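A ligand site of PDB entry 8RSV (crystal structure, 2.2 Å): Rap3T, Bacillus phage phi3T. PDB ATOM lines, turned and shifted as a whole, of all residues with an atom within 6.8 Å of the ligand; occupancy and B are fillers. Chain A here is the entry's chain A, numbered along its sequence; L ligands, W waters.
O2 of the ligand is in hydrogen-bond range of NZ of Lys 330, 2.9 Å away. An oxygen (O6) of the ligand lies within hydrogen-bond range of the backbone NH (N) of Leu 117, at 2.9 Å. O6 of the ligand is in hydrogen-bond range of N of Tyr 116 (3.2 Å).
O5 of the ligand sits close to OE1 of Glu 115. Gln 113 touches the ligand. Tyr 114 touches the ligand (O to C6, 3.4 Å). Ile 300 touches the ligand (CD1 to C6, 3.8 Å). O of Leu 329 touches C8 of the ligand, at 3.8 Å. OG of Ser 331 touches C9 of the ligand, 3.6 Å away. Hydrophobic or aromatic side chains that line the ligand: Leu 117 and Ile 300. The nearest printed residue that does not touch the ligand is Glu 299 (4.4 Å).
Water W1 lies within hydrogen-bond range of an oxygen (O6) of the ligand (2.8 Å), the side-chain carboxylate (OE1) of Glu 115 (2.9 Å), the backbone NH (N) of Asn 118 (2.9 Å) and the backbone NH (N) of Leu 117 (3.3 Å).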
ATOM      1  N   GLN A 113     -32.576  12.132 -22.875  1.00  0.00           N
ATOM      2  CA  GLN A 113     -32.396  10.689 -22.962  1.00  0.00           C
ATOM      3  C   GLN A 113     -31.069  10.293 -23.575  1.00  0.00           C
ATOM      4  O   GLN A 113     -30.941   9.151 -24.017  1.00  0.00           O
ATOM      5  CB  GLN A 113     -33.501  10.041 -23.783  1.00  0.00           C
ATOM      6  CG  GLN A 113     -34.898  10.469 -23.402  1.00  0.00           C
ATOM      7  CD  GLN A 113     -35.157  10.226 -21.956  1.00  0.00           C
ATOM      8  OE1 GLN A 113     -35.510  11.140 -21.211  1.00  0.00           O
ATOM      9  NE2 GLN A 113     -34.974   8.986 -21.532  1.00  0.00           N
ATOM     10  N   TYR A 114     -30.107  11.213 -23.696  1.00  0.00           N
ATOM     11  CA  TYR A 114     -28.818  10.904 -24.324  1.00  0.00           C
ATOM     12  C   TYR A 114     -28.969  10.518 -25.805  1.00  0.00           C
ATOM     13  O   TYR A 114     -28.091   9.828 -26.365  1.00  0.00           O
ATOM     14  CB  TYR A 114     -28.079   9.784 -23.594  1.00  0.00           C
ATOM     15  CG  TYR A 114     -27.716   9.972 -22.132  1.00  0.00           C
ATOM     16  CD1 TYR A 114     -26.584  10.692 -21.764  1.00  0.00           C
ATOM     17  CD2 TYR A 114     -28.465   9.356 -21.112  1.00  0.00           C
ATOM     18  CE1 TYR A 114     -26.210  10.824 -20.419  1.00  0.00           C
ATOM     19  CE2 TYR A 114     -28.100   9.482 -19.764  1.00  0.00           C
ATOM     20  CZ  TYR A 114     -26.979  10.221 -19.425  1.00  0.00           C
ATOM     21  OH  TYR A 114     -26.616  10.385 -18.116  1.00  0.00           O
ATOM     22  N   GLU A 115     -30.094  10.879 -26.449  1.00  0.00           N
ATOM     23  CA  GLU A 115     -30.314  10.599 -27.868  1.00  0.00           C
ATOM     24  C   GLU A 115     -29.849  11.834 -28.625  1.00  0.00           C
ATOM     25  O   GLU A 115     -30.658  12.667 -29.097  1.00  0.00           O
ATOM     26  CB  GLU A 115     -31.785  10.334 -28.156  1.00  0.00           C
ATOM     27  CG  GLU A 115     -32.369   9.079 -27.579  1.00  0.00           C
ATOM     28  CD  GLU A 115     -31.935   7.825 -28.278  1.00  0.00           C
ATOM     29  OE1 GLU A 115     -31.210   7.888 -29.308  1.00  0.00           O
ATOM     30  OE2 GLU A 115     -32.328   6.760 -27.785  1.00  0.00           O
ATOM     31  N   TYR A 116     -28.533  11.955 -28.749  1.00  0.00           N
ATOM     32  CA  TYR A 116     -27.948  13.203 -29.214  1.00  0.00           C
ATOM     33  C   TYR A 116     -28.268  13.459 -30.686  1.00  0.00           C
ATOM     34  O   TYR A 116     -28.717  14.549 -31.035  1.00  0.00           O
ATOM     35  CB  TYR A 116     -26.445  13.215 -28.939  1.00  0.00           C
ATOM     36  CG  TYR A 116     -26.145  13.315 -27.442  1.00  0.00           C
ATOM     37  CD1 TYR A 116     -26.759  14.276 -26.682  1.00  0.00           C
ATOM     38  CD2 TYR A 116     -25.270  12.430 -26.806  1.00  0.00           C
ATOM     39  CE1 TYR A 116     -26.542  14.394 -25.359  1.00  0.00           C
ATOM     40  CE2 TYR A 116     -25.027  12.540 -25.424  1.00  0.00           C
ATOM     41  CZ  TYR A 116     -25.665  13.526 -24.718  1.00  0.00           C
ATOM     42  OH  TYR A 116     -25.490  13.675 -23.365  1.00  0.00           O
ATOM     43  N   LEU A 117     -28.155  12.437 -31.547  1.00  0.00           N
ATOM     44  CA  LEU A 117     -28.408  12.663 -32.971  1.00  0.00           C
ATOM     45  C   LEU A 117     -29.873  13.030 -33.229  1.00  0.00           C
ATOM     46  O   LEU A 117     -30.151  13.921 -34.032  1.00  0.00           O
ATOM     47  CB  LEU A 117     -27.993  11.450 -33.797  1.00  0.00           C
ATOM     48  CG  LEU A 117     -26.461  11.184 -33.784  1.00  0.00           C
ATOM     49  CD1 LEU A 117     -25.983  10.098 -34.757  1.00  0.00           C
ATOM     50  CD2 LEU A 117     -25.728  12.484 -34.060  1.00  0.00           C
ATOM     51  N   ASN A 118     -30.811  12.344 -32.576  1.00  0.00           N
ATOM     52  CA  ASN A 118     -32.228  12.711 -32.681  1.00  0.00           C
ATOM     53  C   ASN A 118     -32.449  14.141 -32.242  1.00  0.00           C
ATOM     54  O   ASN A 118     -33.235  14.866 -32.842  1.00  0.00           O
ATOM     55  CB  ASN A 118     -33.068  11.790 -31.818  1.00  0.00           C
ATOM     56  CG  ASN A 118     -33.164  10.405 -32.384  1.00  0.00           C
ATOM     57  OD1 ASN A 118     -32.719  10.146 -33.496  1.00  0.00           O
ATOM     58  ND2 ASN A 118     -33.707   9.499 -31.604  1.00  0.00           N
ATOM     59  N   ALA A 119     -31.759  14.548 -31.163  1.00  0.00           N
ATOM     60  CA  ALA A 119     -31.936  15.867 -30.579  1.00  0.00           C
ATOM     61  C   ALA A 119     -31.487  16.965 -31.540  1.00  0.00           C
ATOM     62  O   ALA A 119     -32.225  17.934 -31.763  1.00  0.00           O
ATOM     63  CB  ALA A 119     -31.189  15.943 -29.252  1.00  0.00           C
ATOM     64  N   GLU A 299     -27.275   3.366 -18.235  1.00  0.00           N
ATOM     65  CA  GLU A 299     -26.282   2.497 -18.857  1.00  0.00           C
ATOM     66  C   GLU A 299     -25.034   3.276 -19.256  1.00  0.00           C
ATOM     67  O   GLU A 299     -23.894   2.791 -19.112  1.00  0.00           O
ATOM     68  CB  GLU A 299     -26.870   1.831 -20.085  1.00  0.00           C
ATOM     69  CG  GLU A 299     -26.039   0.622 -20.594  1.00  0.00           C
ATOM     70  CD  GLU A 299     -26.507   0.095 -21.963  1.00  0.00           C
ATOM     71  OE1 GLU A 299     -26.646   0.884 -22.934  1.00  0.00           O
ATOM     72  OE2 GLU A 299     -26.819  -1.090 -22.044  1.00  0.00           O
ATOM     73  N   ILE A 300     -25.233   4.486 -19.810  1.00  0.00           N
ATOM     74  CA  ILE A 300     -24.121   5.247 -20.347  1.00  0.00           C
ATOM     75  C   ILE A 300     -23.163   5.653 -19.225  1.00  0.00           C
ATOM     76  O   ILE A 300     -21.940   5.557 -19.370  1.00  0.00           O
ATOM     77  CB  ILE A 300     -24.611   6.467 -21.131  1.00  0.00           C
ATOM     78  CG1 ILE A 300     -25.037   6.053 -22.534  1.00  0.00           C
ATOM     79  CG2 ILE A 300     -23.519   7.531 -21.177  1.00  0.00           C
ATOM     80  CD1 ILE A 300     -25.899   7.081 -23.175  1.00  0.00           C
ATOM     81  N   ASN A 325     -15.635   2.166 -28.088  1.00  0.00           N
ATOM     82  CA  ASN A 325     -16.474   1.969 -29.259  1.00  0.00           C
ATOM     83  C   ASN A 325     -17.947   2.219 -28.949  1.00  0.00           C
ATOM     84  O   ASN A 325     -18.670   2.824 -29.756  1.00  0.00           O
ATOM     85  CB  ASN A 325     -16.275   0.558 -29.804  1.00  0.00           C
ATOM     86  CG  ASN A 325     -17.032   0.317 -31.085  1.00  0.00           C
ATOM     87  OD1 ASN A 325     -16.669   0.823 -32.138  1.00  0.00           O
ATOM     88  ND2 ASN A 325     -18.081  -0.514 -31.004  1.00  0.00           N
ATOM     89  N   TYR A 326     -18.421   1.737 -27.801  1.00  0.00           N
ATOM     90  CA  TYR A 326     -19.798   1.997 -27.415  1.00  0.00           C
ATOM     91  C   TYR A 326     -20.088   3.501 -27.346  1.00  0.00           C
ATOM     92  O   TYR A 326     -21.063   3.979 -27.926  1.00  0.00           O
ATOM     93  CB  TYR A 326     -20.078   1.297 -26.094  1.00  0.00           C
ATOM     94  CG  TYR A 326     -21.404   1.582 -25.435  1.00  0.00           C
ATOM     95  CD1 TYR A 326     -21.555   2.692 -24.591  1.00  0.00           C
ATOM     96  CD2 TYR A 326     -22.466   0.691 -25.557  1.00  0.00           C
ATOM     97  CE1 TYR A 326     -22.741   2.946 -23.947  1.00  0.00           C
ATOM     98  CE2 TYR A 326     -23.681   0.937 -24.900  1.00  0.00           C
ATOM     99  CZ  TYR A 326     -23.800   2.073 -24.098  1.00  0.00           C
ATOM    100  OH  TYR A 326     -24.973   2.338 -23.426  1.00  0.00           O
ATOM    101  N   GLU A 328     -18.660   5.907 -28.805  1.00  0.00           N
ATOM    102  CA  GLU A 328     -18.669   6.466 -30.143  1.00  0.00           C
ATOM    103  C   GLU A 328     -19.991   6.176 -30.838  1.00  0.00           C
ATOM    104  O   GLU A 328     -20.545   7.056 -31.526  1.00  0.00           O
ATOM    105  CB  GLU A 328     -17.509   5.904 -30.963  1.00  0.00           C
ATOM    106  CG  GLU A 328     -17.356   6.543 -32.339  1.00  0.00           C
ATOM    107  CD  GLU A 328     -16.249   5.896 -33.169  1.00  0.00           C
ATOM    108  OE1 GLU A 328     -15.450   5.121 -32.614  1.00  0.00           O
ATOM    109  OE2 GLU A 328     -16.172   6.170 -34.386  1.00  0.00           O
ATOM    110  N   LEU A 329     -20.523   4.981 -30.663  1.00  0.00           N
ATOM    111  CA  LEU A 329     -21.840   4.671 -31.220  1.00  0.00           C
ATOM    112  C   LEU A 329     -22.937   5.487 -30.557  1.00  0.00           C
ATOM    113  O   LEU A 329     -23.993   5.693 -31.178  1.00  0.00           O
ATOM    114  CB  LEU A 329     -22.148   3.176 -31.086  1.00  0.00           C
ATOM    115  CG  LEU A 329     -21.285   2.257 -31.963  1.00  0.00           C
ATOM    116  CD1 LEU A 329     -21.686   0.788 -31.800  1.00  0.00           C
ATOM    117  CD2 LEU A 329     -21.340   2.721 -33.447  1.00  0.00           C
ATOM    118  N   LYS A 330     -22.709   6.000 -29.354  1.00  0.00           N
ATOM    119  CA  LYS A 330     -23.622   6.935 -28.723  1.00  0.00           C
ATOM    120  C   LYS A 330     -23.339   8.372 -29.094  1.00  0.00           C
ATOM    121  O   LYS A 330     -23.981   9.265 -28.523  1.00  0.00           O
ATOM    122  CB  LYS A 330     -23.595   6.825 -27.203  1.00  0.00           C
ATOM    123  CG  LYS A 330     -23.893   5.454 -26.655  1.00  0.00           C
ATOM    124  CD  LYS A 330     -25.333   5.141 -26.889  1.00  0.00           C
ATOM    125  CE  LYS A 330     -25.704   3.758 -26.436  1.00  0.00           C
ATOM    126  NZ  LYS A 330     -27.081   3.365 -26.852  1.00  0.00           N
ATOM    127  N   SER A 331     -22.439   8.620 -30.054  1.00  0.00           N
ATOM    128  CA  SER A 331     -22.155   9.976 -30.510  1.00  0.00           C
ATOM    129  C   SER A 331     -21.655  10.821 -29.348  1.00  0.00           C
ATOM    130  O   SER A 331     -21.945  12.030 -29.254  1.00  0.00           O
ATOM    131  CB  SER A 331     -23.396  10.632 -31.129  1.00  0.00           C
ATOM    132  OG  SER A 331     -23.706  10.002 -32.352  1.00  0.00           O
ATOM    133  N   MET A 332     -20.903  10.187 -28.441  1.00  0.00           N
ATOM    134  CA  MET A 332     -20.352  10.885 -27.292  1.00  0.00           C
ATOM    135  C   MET A 332     -18.825  10.942 -27.425  1.00  0.00           C
ATOM    136  O   MET A 332     -18.071  10.358 -26.636  1.00  0.00           O
ATOM    137  CB  MET A 332     -20.799  10.190 -26.023  1.00  0.00           C
ATOM    138  CG  MET A 332     -22.233  10.513 -25.698  1.00  0.00           C
ATOM    139  SD  MET A 332     -22.903   9.511 -24.373  1.00  0.00           S
ATOM    140  CE  MET A 332     -22.434  10.560 -22.983  1.00  0.00           C
HETATM  141  C1  LIG L   1     -26.370   1.623 -29.819  1.00  0.00           C
HETATM  142  C2  LIG L   1     -26.634   2.912 -30.548  1.00  0.00           C
HETATM  143  C3  LIG L   1     -27.745   4.984 -30.408  1.00  0.00           C
HETATM  144  C4  LIG L   1     -28.649   5.812 -29.516  1.00  0.00           C
HETATM  145  C5  LIG L   1     -28.293   5.696 -28.068  1.00  0.00           C
HETATM  146  C6  LIG L   1     -28.507   6.454 -25.823  1.00  0.00           C
HETATM  147  C7  LIG L   1     -29.345   5.662 -24.873  1.00  0.00           C
HETATM  148  O1  LIG L   1     -25.188   1.567 -29.039  1.00  0.00           O
HETATM  149  O2  LIG L   1     -27.283   3.840 -29.689  1.00  0.00           O
HETATM  150  O3  LIG L   1     -29.028   6.507 -27.153  1.00  0.00           O
HETATM  151  O4  LIG L   1     -28.730   4.471 -24.389  1.00  0.00           O
HETATM  152  O5  LIG L   1     -28.411   7.167 -29.908  1.00  0.00           O
HETATM  153  C8  LIG L   1     -27.029   7.576 -29.824  1.00  0.00           C
HETATM  154  C9  LIG L   1     -26.657   8.594 -30.862  1.00  0.00           C
HETATM  155  O6  LIG L   1     -27.422   9.780 -30.807  1.00  0.00           O
HETATM  156  O   HOH W   1     -30.140   9.808 -31.239  1.00  0.00           O
